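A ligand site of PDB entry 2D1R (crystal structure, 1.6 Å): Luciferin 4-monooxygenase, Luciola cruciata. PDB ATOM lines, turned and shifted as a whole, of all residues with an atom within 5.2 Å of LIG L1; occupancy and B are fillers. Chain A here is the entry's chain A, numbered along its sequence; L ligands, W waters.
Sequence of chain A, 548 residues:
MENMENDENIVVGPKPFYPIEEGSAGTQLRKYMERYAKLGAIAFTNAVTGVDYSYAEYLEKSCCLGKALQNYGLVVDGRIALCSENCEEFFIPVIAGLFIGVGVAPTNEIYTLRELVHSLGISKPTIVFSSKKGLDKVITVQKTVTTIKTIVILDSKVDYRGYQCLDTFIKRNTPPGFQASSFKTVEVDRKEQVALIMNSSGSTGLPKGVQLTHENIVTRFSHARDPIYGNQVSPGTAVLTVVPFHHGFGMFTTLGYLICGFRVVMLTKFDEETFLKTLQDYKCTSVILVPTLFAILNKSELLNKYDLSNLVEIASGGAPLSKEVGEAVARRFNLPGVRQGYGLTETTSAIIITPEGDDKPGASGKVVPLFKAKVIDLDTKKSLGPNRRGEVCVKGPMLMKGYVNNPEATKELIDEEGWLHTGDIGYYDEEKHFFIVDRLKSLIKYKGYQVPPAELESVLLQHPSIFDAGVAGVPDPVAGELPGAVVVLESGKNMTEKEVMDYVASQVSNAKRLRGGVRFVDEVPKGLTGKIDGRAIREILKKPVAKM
An oxygen (O6) of LIG L1 is in hydrogen-bond range of the side-chain carboxylate (OD1) of Asp 424 (2.7 Å).
O1 of LIG L1 sits at hydrogen-bond distance from N of Thr 345, 2.8 Å away.
OG1 of Thr 345 lies within hydrogen-bond range of O1 of LIG L1, 2.7 Å away.
A ring nitrogen (NE2) of His 247 lies within hydrogen-bond range of an oxygen (O3) of LIG L1 (2.7 Å).
OG of Ser 200 sits at hydrogen-bond distance from O2 of LIG L1 (2.7 Å).
A nitrogen (N3) of LIG L1 sits at hydrogen-bond distance from the backbone carbonyl oxygen (O) of Gly 341 (2.8 Å).
O3 of LIG L1 lies within hydrogen-bond range of N of Ser 201.
The side-chain hydroxyl of Ser 201 sits at hydrogen-bond distance from an oxygen (O3) of LIG L1, at 2.9 Å.
The side-chain amino group of Lys 531 is in salt-bridge range of an oxygen (O3) of LIG L1, 3.0 Å away.
A nitrogen (N2) of LIG L1 lies within hydrogen-bond range of the backbone NH of Gly 318 (3.3 Å).
NE2 of Gln 340 sits close to N3 of LIG L1 (3.3 Å).
N of Gly 318 sits close to S2 of LG2 L2, 3.7 Å away.
O1 of LIG L1 lies close to O1 of LG2 L2 (2.9 Å).
The side-chain carboxylate (OD1) of Asp 424 is in hydrogen-bond range of the side-chain hydroxyl (OH) of Tyr 342.
N of Asp 424 sits at hydrogen-bond distance from OG1 of Thr 422.
A ring nitrogen (NE2) of His 247 sits at hydrogen-bond distance from the side-chain hydroxyl (OG) of Ser 201 (3.2 Å).
N of Gly 341 is in hydrogen-bond range of O of Ser 316, at 3.2 Å.
The side-chain hydroxyl (OG) of Ser 201 sits at hydrogen-bond distance from the side-chain hydroxyl (OG1) of Thr 529 (2.8 Å).
OG1 of Thr 529 is in hydrogen-bond range of NZ of Lys 531 (3.3 Å).
The side-chain hydroxyl (OH) of Tyr 342 lies close to the side-chain hydroxyl (OG1) of Thr 422 (3.3 Å).
The backbone NH (N) of Ile 436 lies within hydrogen-bond range of the side-chain hydroxyl (OG) of Ser 364 (3.3 Å).
Ala 319 touches LIG L1 (C to C9, 3.5 Å).
Pro 320 touches LIG L1.
CD1 of Tyr 342 touches C7 of LIG L1 (3.6 Å).
Gly 343 touches LIG L1.
CG of Leu 344 touches O6 of LIG L1 (3.4 Å).
Ile 436 touches LIG L1.
Arg 439 touches LIG L1 (CG to O7, 3.3 Å).
Hydrophobic or aromatic side chains within 4 Å of LIG L1: His 247, Pro 320, Tyr 342, Leu 344 and Ile 436.
Of the 23 residues printed, 16 come within 4 Å of LIG L1.
The nearest printed residue that does not touch LIG L1 is Thr 422 (4.1 Å).
Water W1 lies within hydrogen-bond range of O2 of LIG L1, OE1 of Glu 346 and OG of Ser 200.
Water W6 lies within hydrogen-bond range of the side-chain amide nitrogen (NE2) of Gln 340, the backbone NH (N) of Leu 321 and a nitrogen (N4) of LIG L1.
Water W2 lies within hydrogen-bond range of the backbone carbonyl oxygen of Thr 422 (2.9 Å), the side-chain carboxylate of Asp 424 (3.0 Å) and an oxygen (O6) of LIG L1 (3.5 Å).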
ATOM      1  N   SER A 200      12.681  22.700  -6.858  1.00  0.00           N
ATOM      2  CA  SER A 200      13.519  22.699  -5.655  1.00  0.00           C
ATOM      3  C   SER A 200      14.975  22.983  -6.011  1.00  0.00           C
ATOM      4  O   SER A 200      15.380  22.861  -7.180  1.00  0.00           O
ATOM      5  CB  SER A 200      13.468  21.309  -4.992  1.00  0.00           C
ATOM      6  OG  SER A 200      12.216  21.079  -4.357  1.00  0.00           O
ATOM      7  N   SER A 201      15.750  23.352  -5.000  1.00  0.00           N
ATOM      8  CA  SER A 201      17.201  23.477  -5.144  1.00  0.00           C
ATOM      9  C   SER A 201      17.860  22.367  -4.329  1.00  0.00           C
ATOM     10  O   SER A 201      17.269  21.856  -3.374  1.00  0.00           O
ATOM     11  CB  SER A 201      17.692  24.814  -4.626  1.00  0.00           C
ATOM     12  OG  SER A 201      17.206  25.066  -3.318  1.00  0.00           O
ATOM     13  N   HIS A 247      13.172  30.478  -7.350  1.00  0.00           N
ATOM     14  CA  HIS A 247      12.925  29.484  -6.293  1.00  0.00           C
ATOM     15  C   HIS A 247      11.798  29.958  -5.367  1.00  0.00           C
ATOM     16  O   HIS A 247      11.599  31.149  -5.182  1.00  0.00           O
ATOM     17  CB  HIS A 247      14.230  29.281  -5.513  1.00  0.00           C
ATOM     18  CG  HIS A 247      14.173  28.218  -4.470  1.00  0.00           C
ATOM     19  ND1 HIS A 247      13.660  28.441  -3.212  1.00  0.00           N
ATOM     20  CD2 HIS A 247      14.616  26.934  -4.472  1.00  0.00           C
ATOM     21  CE1 HIS A 247      13.746  27.331  -2.495  1.00  0.00           C
ATOM     22  NE2 HIS A 247      14.331  26.398  -3.241  1.00  0.00           N
ATOM     23  N   SER A 316      15.866  34.963   8.044  1.00  0.00           N
ATOM     24  CA  SER A 316      16.615  33.897   7.408  1.00  0.00           C
ATOM     25  C   SER A 316      15.672  32.807   6.970  1.00  0.00           C
ATOM     26  O   SER A 316      14.587  32.645   7.546  1.00  0.00           O
ATOM     27  CB  SER A 316      17.592  33.275   8.389  1.00  0.00           C
ATOM     28  OG  SER A 316      18.378  32.259   7.768  1.00  0.00           O
ATOM     29  N   GLY A 317      16.115  32.051   5.984  1.00  0.00           N
ATOM     30  CA  GLY A 317      15.387  30.876   5.530  1.00  0.00           C
ATOM     31  C   GLY A 317      16.239  30.051   4.579  1.00  0.00           C
ATOM     32  O   GLY A 317      17.407  30.364   4.297  1.00  0.00           O
ATOM     33  N   GLY A 318      15.652  28.959   4.104  1.00  0.00           N
ATOM     34  CA  GLY A 318      16.274  28.141   3.072  1.00  0.00           C
ATOM     35  C   GLY A 318      17.139  26.987   3.546  1.00  0.00           C
ATOM     36  O   GLY A 318      17.173  25.961   2.884  1.00  0.00           O
ATOM     37  N   ALA A 319      17.841  27.168   4.661  1.00  0.00           N
ATOM     38  CA  ALA A 319      18.787  26.177   5.160  1.00  0.00           C
ATOM     39  C   ALA A 319      19.004  26.410   6.642  1.00  0.00           C
ATOM     40  O   ALA A 319      18.670  27.486   7.152  1.00  0.00           O
ATOM     41  CB  ALA A 319      20.106  26.275   4.384  1.00  0.00           C
ATOM     42  N   PRO A 320      19.584  25.443   7.351  1.00  0.00           N
ATOM     43  CA  PRO A 320      19.855  25.636   8.792  1.00  0.00           C
ATOM     44  C   PRO A 320      20.735  26.861   9.054  1.00  0.00           C
ATOM     45  O   PRO A 320      21.727  27.081   8.360  1.00  0.00           O
ATOM     46  CB  PRO A 320      20.566  24.342   9.197  1.00  0.00           C
ATOM     47  CG  PRO A 320      20.073  23.329   8.164  1.00  0.00           C
ATOM     48  CD  PRO A 320      19.992  24.108   6.887  1.00  0.00           C
ATOM     49  N   LEU A 321      20.326  27.666  10.034  1.00  0.00           N
ATOM     50  CA  LEU A 321      21.119  28.805  10.500  1.00  0.00           C
ATOM     51  C   LEU A 321      21.676  28.445  11.865  1.00  0.00           C
ATOM     52  O   LEU A 321      20.919  28.027  12.731  1.00  0.00           O
ATOM     53  CB  LEU A 321      20.230  30.051  10.629  1.00  0.00           C
ATOM     54  CG  LEU A 321      20.867  31.302  11.261  1.00  0.00           C
ATOM     55  CD1 LEU A 321      22.013  31.862  10.431  1.00  0.00           C
ATOM     56  CD2 LEU A 321      19.812  32.369  11.506  1.00  0.00           C
ATOM     57  N   GLN A 340      12.722  33.806  11.396  1.00  0.00           N
ATOM     58  CA  GLN A 340      13.011  32.649  10.544  1.00  0.00           C
ATOM     59  C   GLN A 340      11.732  32.123   9.900  1.00  0.00           C
ATOM     60  O   GLN A 340      10.629  32.314  10.414  1.00  0.00           O
ATOM     61  CB  GLN A 340      13.711  31.559  11.354  1.00  0.00           C
ATOM     62  CG  GLN A 340      14.359  30.484  10.495  1.00  0.00           C
ATOM     63  CD  GLN A 340      15.520  29.763  11.194  1.00  0.00           C
ATOM     64  OE1 GLN A 340      15.731  29.906  12.406  1.00  0.00           O
ATOM     65  NE2 GLN A 340      16.256  28.989  10.430  1.00  0.00           N
ATOM     66  N   GLY A 341      11.916  31.468   8.763  1.00  0.00           N
ATOM     67  CA  GLY A 341      10.841  30.761   8.090  1.00  0.00           C
ATOM     68  C   GLY A 341      11.388  29.437   7.582  1.00  0.00           C
ATOM     69  O   GLY A 341      12.545  29.363   7.146  1.00  0.00           O
ATOM     70  N   TYR A 342      10.542  28.413   7.648  1.00  0.00           N
ATOM     71  CA  TYR A 342      10.883  27.073   7.193  1.00  0.00           C
ATOM     72  C   TYR A 342       9.747  26.563   6.332  1.00  0.00           C
ATOM     73  O   TYR A 342       8.582  26.614   6.730  1.00  0.00           O
ATOM     74  CB  TYR A 342      11.067  26.141   8.394  1.00  0.00           C
ATOM     75  CG  TYR A 342      10.921  24.661   8.049  1.00  0.00           C
ATOM     76  CD1 TYR A 342      11.945  23.986   7.395  1.00  0.00           C
ATOM     77  CD2 TYR A 342       9.776  23.966   8.372  1.00  0.00           C
ATOM     78  CE1 TYR A 342      11.810  22.612   7.061  1.00  0.00           C
ATOM     79  CE2 TYR A 342       9.611  22.625   8.040  1.00  0.00           C
ATOM     80  CZ  TYR A 342      10.643  21.963   7.402  1.00  0.00           C
ATOM     81  OH  TYR A 342      10.491  20.647   7.081  1.00  0.00           O
ATOM     82  N   GLY A 343      10.101  26.120   5.132  1.00  0.00           N
ATOM     83  CA  GLY A 343       9.136  25.515   4.238  1.00  0.00           C
ATOM     84  C   GLY A 343       9.874  24.763   3.144  1.00  0.00           C
ATOM     85  O   GLY A 343      11.106  24.687   3.141  1.00  0.00           O
ATOM     86  N   LEU A 344       9.087  24.199   2.236  1.00  0.00           N
ATOM     87  CA  LEU A 344       9.613  23.438   1.100  1.00  0.00           C
ATOM     88  C   LEU A 344       8.978  23.977  -0.162  1.00  0.00           C
ATOM     89  O   LEU A 344       7.881  24.568  -0.107  1.00  0.00           O
ATOM     90  CB  LEU A 344       9.208  21.972   1.223  1.00  0.00           C
ATOM     91  CG  LEU A 344       9.892  21.017   2.212  1.00  0.00           C
ATOM     92  CD1 LEU A 344       9.625  21.394   3.644  1.00  0.00           C
ATOM     93  CD2 LEU A 344       9.399  19.613   1.922  1.00  0.00           C
ATOM     94  N   THR A 345       9.609  23.742  -1.325  1.00  0.00           N
ATOM     95  CA  THR A 345       8.969  24.116  -2.590  1.00  0.00           C
ATOM     96  C   THR A 345       7.549  23.511  -2.658  1.00  0.00           C
ATOM     97  O   THR A 345       6.590  24.183  -3.058  1.00  0.00           O
ATOM     98  CB  THR A 345       9.842  23.608  -3.754  1.00  0.00           C
ATOM     99  OG1 THR A 345      11.066  24.351  -3.751  1.00  0.00           O
ATOM    100  CG2 THR A 345       9.217  23.993  -5.103  1.00  0.00           C
ATOM    101  N   GLU A 346       7.422  22.272  -2.202  1.00  0.00           N
ATOM    102  CA  GLU A 346       6.156  21.539  -2.228  1.00  0.00           C
ATOM    103  C   GLU A 346       5.105  22.042  -1.236  1.00  0.00           C
ATOM    104  O   GLU A 346       3.957  21.602  -1.306  1.00  0.00           O
ATOM    105  CB  GLU A 346       6.428  20.027  -1.994  1.00  0.00           C
ATOM    106  CG  GLU A 346       7.279  19.352  -3.078  1.00  0.00           C
ATOM    107  CD  GLU A 346       8.787  19.357  -2.817  1.00  0.00           C
ATOM    108  OE1 GLU A 346       9.304  20.204  -2.036  1.00  0.00           O
ATOM    109  OE2 GLU A 346       9.471  18.512  -3.462  1.00  0.00           O
ATOM    110  N   SER A 364      12.738  27.730  14.766  1.00  0.00           N
ATOM    111  CA  SER A 364      12.375  28.104  13.418  1.00  0.00           C
ATOM    112  C   SER A 364      11.030  28.841  13.390  1.00  0.00           C
ATOM    113  O   SER A 364      10.686  29.506  12.412  1.00  0.00           O
ATOM    114  CB  SER A 364      12.327  26.848  12.513  1.00  0.00           C
ATOM    115  OG  SER A 364      13.521  26.089  12.655  1.00  0.00           O
ATOM    116  N   THR A 422       8.148  15.818   5.136  1.00  0.00           N
ATOM    117  CA  THR A 422       9.130  16.811   4.649  1.00  0.00           C
ATOM    118  C   THR A 422      10.517  16.260   4.365  1.00  0.00           C
ATOM    119  O   THR A 422      11.280  16.888   3.626  1.00  0.00           O
ATOM    120  CB  THR A 422       9.333  17.951   5.655  1.00  0.00           C
ATOM    121  OG1 THR A 422       9.834  17.422   6.905  1.00  0.00           O
ATOM    122  CG2 THR A 422       8.044  18.649   5.984  1.00  0.00           C
ATOM    123  N   ASP A 424      12.630  16.161   6.734  1.00  0.00           N
ATOM    124  CA  ASP A 424      13.444  16.898   7.715  1.00  0.00           C
ATOM    125  C   ASP A 424      13.244  16.386   9.115  1.00  0.00           C
ATOM    126  O   ASP A 424      12.121  16.057   9.529  1.00  0.00           O
ATOM    127  CB  ASP A 424      13.123  18.393   7.673  1.00  0.00           C
ATOM    128  CG  ASP A 424      13.405  18.977   6.327  1.00  0.00           C
ATOM    129  OD1 ASP A 424      12.534  19.675   5.757  1.00  0.00           O
ATOM    130  OD2 ASP A 424      14.471  18.724   5.740  1.00  0.00           O
ATOM    131  N   ILE A 436      14.044  22.957  13.492  1.00  0.00           N
ATOM    132  CA  ILE A 436      14.447  22.127  12.352  1.00  0.00           C
ATOM    133  C   ILE A 436      15.944  21.877  12.412  1.00  0.00           C
ATOM    134  O   ILE A 436      16.746  22.810  12.378  1.00  0.00           O
ATOM    135  CB  ILE A 436      14.029  22.785  11.013  1.00  0.00           C
ATOM    136  CG1 ILE A 436      12.541  23.183  11.029  1.00  0.00           C
ATOM    137  CG2 ILE A 436      14.364  21.856   9.814  1.00  0.00           C
ATOM    138  CD1 ILE A 436      11.563  22.016  11.110  1.00  0.00           C
ATOM    139  N   ARG A 439      18.280  17.688   7.221  1.00  0.00           N
ATOM    140  CA  ARG A 439      17.614  16.712   6.379  1.00  0.00           C
ATOM    141  C   ARG A 439      17.909  15.283   6.836  1.00  0.00           C
ATOM    142  O   ARG A 439      19.060  14.951   7.172  1.00  0.00           O
ATOM    143  CB  ARG A 439      18.036  16.894   4.916  1.00  0.00           C
ATOM    144  CG  ARG A 439      17.543  18.201   4.296  1.00  0.00           C
ATOM    145  CD  ARG A 439      18.172  18.516   2.977  1.00  0.00           C
ATOM    146  NE  ARG A 439      19.541  18.999   3.148  1.00  0.00           N
ATOM    147  CZ  ARG A 439      20.402  19.129   2.145  1.00  0.00           C
ATOM    148  NH1 ARG A 439      20.011  18.853   0.917  1.00  0.00           N
ATOM    149  NH2 ARG A 439      21.645  19.555   2.384  1.00  0.00           N
ATOM    150  N   THR A 529      19.900  27.870  -2.582  1.00  0.00           N
ATOM    151  CA  THR A 529      19.405  28.517  -1.363  1.00  0.00           C
ATOM    152  C   THR A 529      20.164  28.109  -0.097  1.00  0.00           C
ATOM    153  O   THR A 529      19.627  28.231   1.025  1.00  0.00           O
ATOM    154  CB  THR A 529      17.890  28.277  -1.169  1.00  0.00           C
ATOM    155  OG1 THR A 529      17.609  26.876  -1.258  1.00  0.00           O
ATOM    156  CG2 THR A 529      17.080  28.912  -2.333  1.00  0.00           C
ATOM    157  N   LYS A 531      21.692  25.088   0.840  1.00  0.00           N
ATOM    158  CA  LYS A 531      21.750  23.730   1.366  1.00  0.00           C
ATOM    159  C   LYS A 531      23.030  23.057   0.907  1.00  0.00           C
ATOM    160  O   LYS A 531      23.422  23.178  -0.260  1.00  0.00           O
ATOM    161  CB  LYS A 531      20.524  22.913   0.943  1.00  0.00           C
ATOM    162  CG  LYS A 531      19.210  23.487   1.466  1.00  0.00           C
ATOM    163  CD  LYS A 531      18.056  22.490   1.342  1.00  0.00           C
ATOM    164  CE  LYS A 531      17.557  22.348  -0.093  1.00  0.00           C
ATOM    165  NZ  LYS A 531      17.193  23.653  -0.724  1.00  0.00           N
HETATM  166  P1  LIG L   1      13.619  23.243  -1.466  1.00  0.00           P
HETATM  167  O1  LIG L   1      12.363  23.993  -1.397  1.00  0.00           O
HETATM  168  O2  LIG L   1      13.289  21.821  -1.954  1.00  0.00           O
HETATM  169  O3  LIG L   1      14.697  23.836  -2.402  1.00  0.00           O
HETATM  170  O4  LIG L   1      14.254  23.038  -0.010  1.00  0.00           O
HETATM  171  C1  LIG L   1      13.405  22.728   1.078  1.00  0.00           C
HETATM  172  C2  LIG L   1      14.330  22.272   2.196  1.00  0.00           C
HETATM  173  O5  LIG L   1      15.152  23.335   2.645  1.00  0.00           O
HETATM  174  C3  LIG L   1      13.601  21.809   3.449  1.00  0.00           C
HETATM  175  O6  LIG L   1      13.122  20.484   3.294  1.00  0.00           O
HETATM  176  C4  LIG L   1      14.700  21.946   4.483  1.00  0.00           C
HETATM  177  O7  LIG L   1      15.588  20.855   4.436  1.00  0.00           O
HETATM  178  C5  LIG L   1      15.461  23.175   4.015  1.00  0.00           C
HETATM  179  N1  LIG L   1      15.020  24.387   4.751  1.00  0.00           N
HETATM  180  C6  LIG L   1      14.184  25.394   4.309  1.00  0.00           C
HETATM  181  N2  LIG L   1      14.050  26.313   5.295  1.00  0.00           N
HETATM  182  C7  LIG L   1      14.810  25.921   6.353  1.00  0.00           C
HETATM  183  C8  LIG L   1      15.064  26.443   7.602  1.00  0.00           C
HETATM  184  N3  LIG L   1      14.530  27.584   8.038  1.00  0.00           N
HETATM  185  N4  LIG L   1      15.905  25.756   8.455  1.00  0.00           N
HETATM  186  C9  LIG L   1      16.476  24.553   8.091  1.00  0.00           C
HETATM  187  N5  LIG L   1      16.238  24.045   6.852  1.00  0.00           N
HETATM  188  C10 LIG L   1      15.415  24.716   6.003  1.00  0.00           C
HETATM  189  O1  LG2 L   2      13.067  25.802   0.709  1.00  0.00           O
HETATM  190  C1  LG2 L   2      12.224  26.688   0.811  1.00  0.00           C
HETATM  191  N1  LG2 L   2      12.213  27.664   1.707  1.00  0.00           N
HETATM  192  C2  LG2 L   2      11.170  28.499   1.575  1.00  0.00           C
HETATM  193  S1  LG2 L   2      10.111  28.223   0.358  1.00  0.00           S
HETATM  194  C3  LG2 L   2      11.070  26.778  -0.143  1.00  0.00           C
HETATM  195  C4  LG2 L   2      10.971  29.678   2.473  1.00  0.00           C
HETATM  196  S2  LG2 L   2      12.090  29.866   3.750  1.00  0.00           S
HETATM  197  C5  LG2 L   2      11.292  31.253   4.145  1.00  0.00           C
HETATM  198  C6  LG2 L   2      11.616  32.125   5.191  1.00  0.00           C
HETATM  199  C7  LG2 L   2      10.141  31.592   3.290  1.00  0.00           C
HETATM  200  N2  LG2 L   2      10.034  30.630   2.371  1.00  0.00           N
HETATM  201  C8  LG2 L   2       9.391  32.740   3.538  1.00  0.00           C
HETATM  202  C9  LG2 L   2       9.743  33.578   4.597  1.00  0.00           C
HETATM  203  C10 LG2 L   2      10.832  33.285   5.412  1.00  0.00           C
HETATM  204  O2  LG2 L   2      11.134  34.141   6.439  1.00  0.00           O
HETATM  205  O   HOH W   1      11.739  20.134  -1.037  1.00  0.00           O
HETATM  206  O   HOH W   2      14.155  17.189   3.226  1.00  0.00           O
HETATM  207  O   HOH W   3      17.560  21.429   6.285  1.00  0.00           O
HETATM  208  O   HOH W   4      12.947  18.785   1.115  1.00  0.00           O
HETATM  209  O   HOH W   5      15.959  25.782   0.450  1.00  0.00           O
HETATM  210  O   HOH W   6      17.463  26.891  11.040  1.00  0.00           O
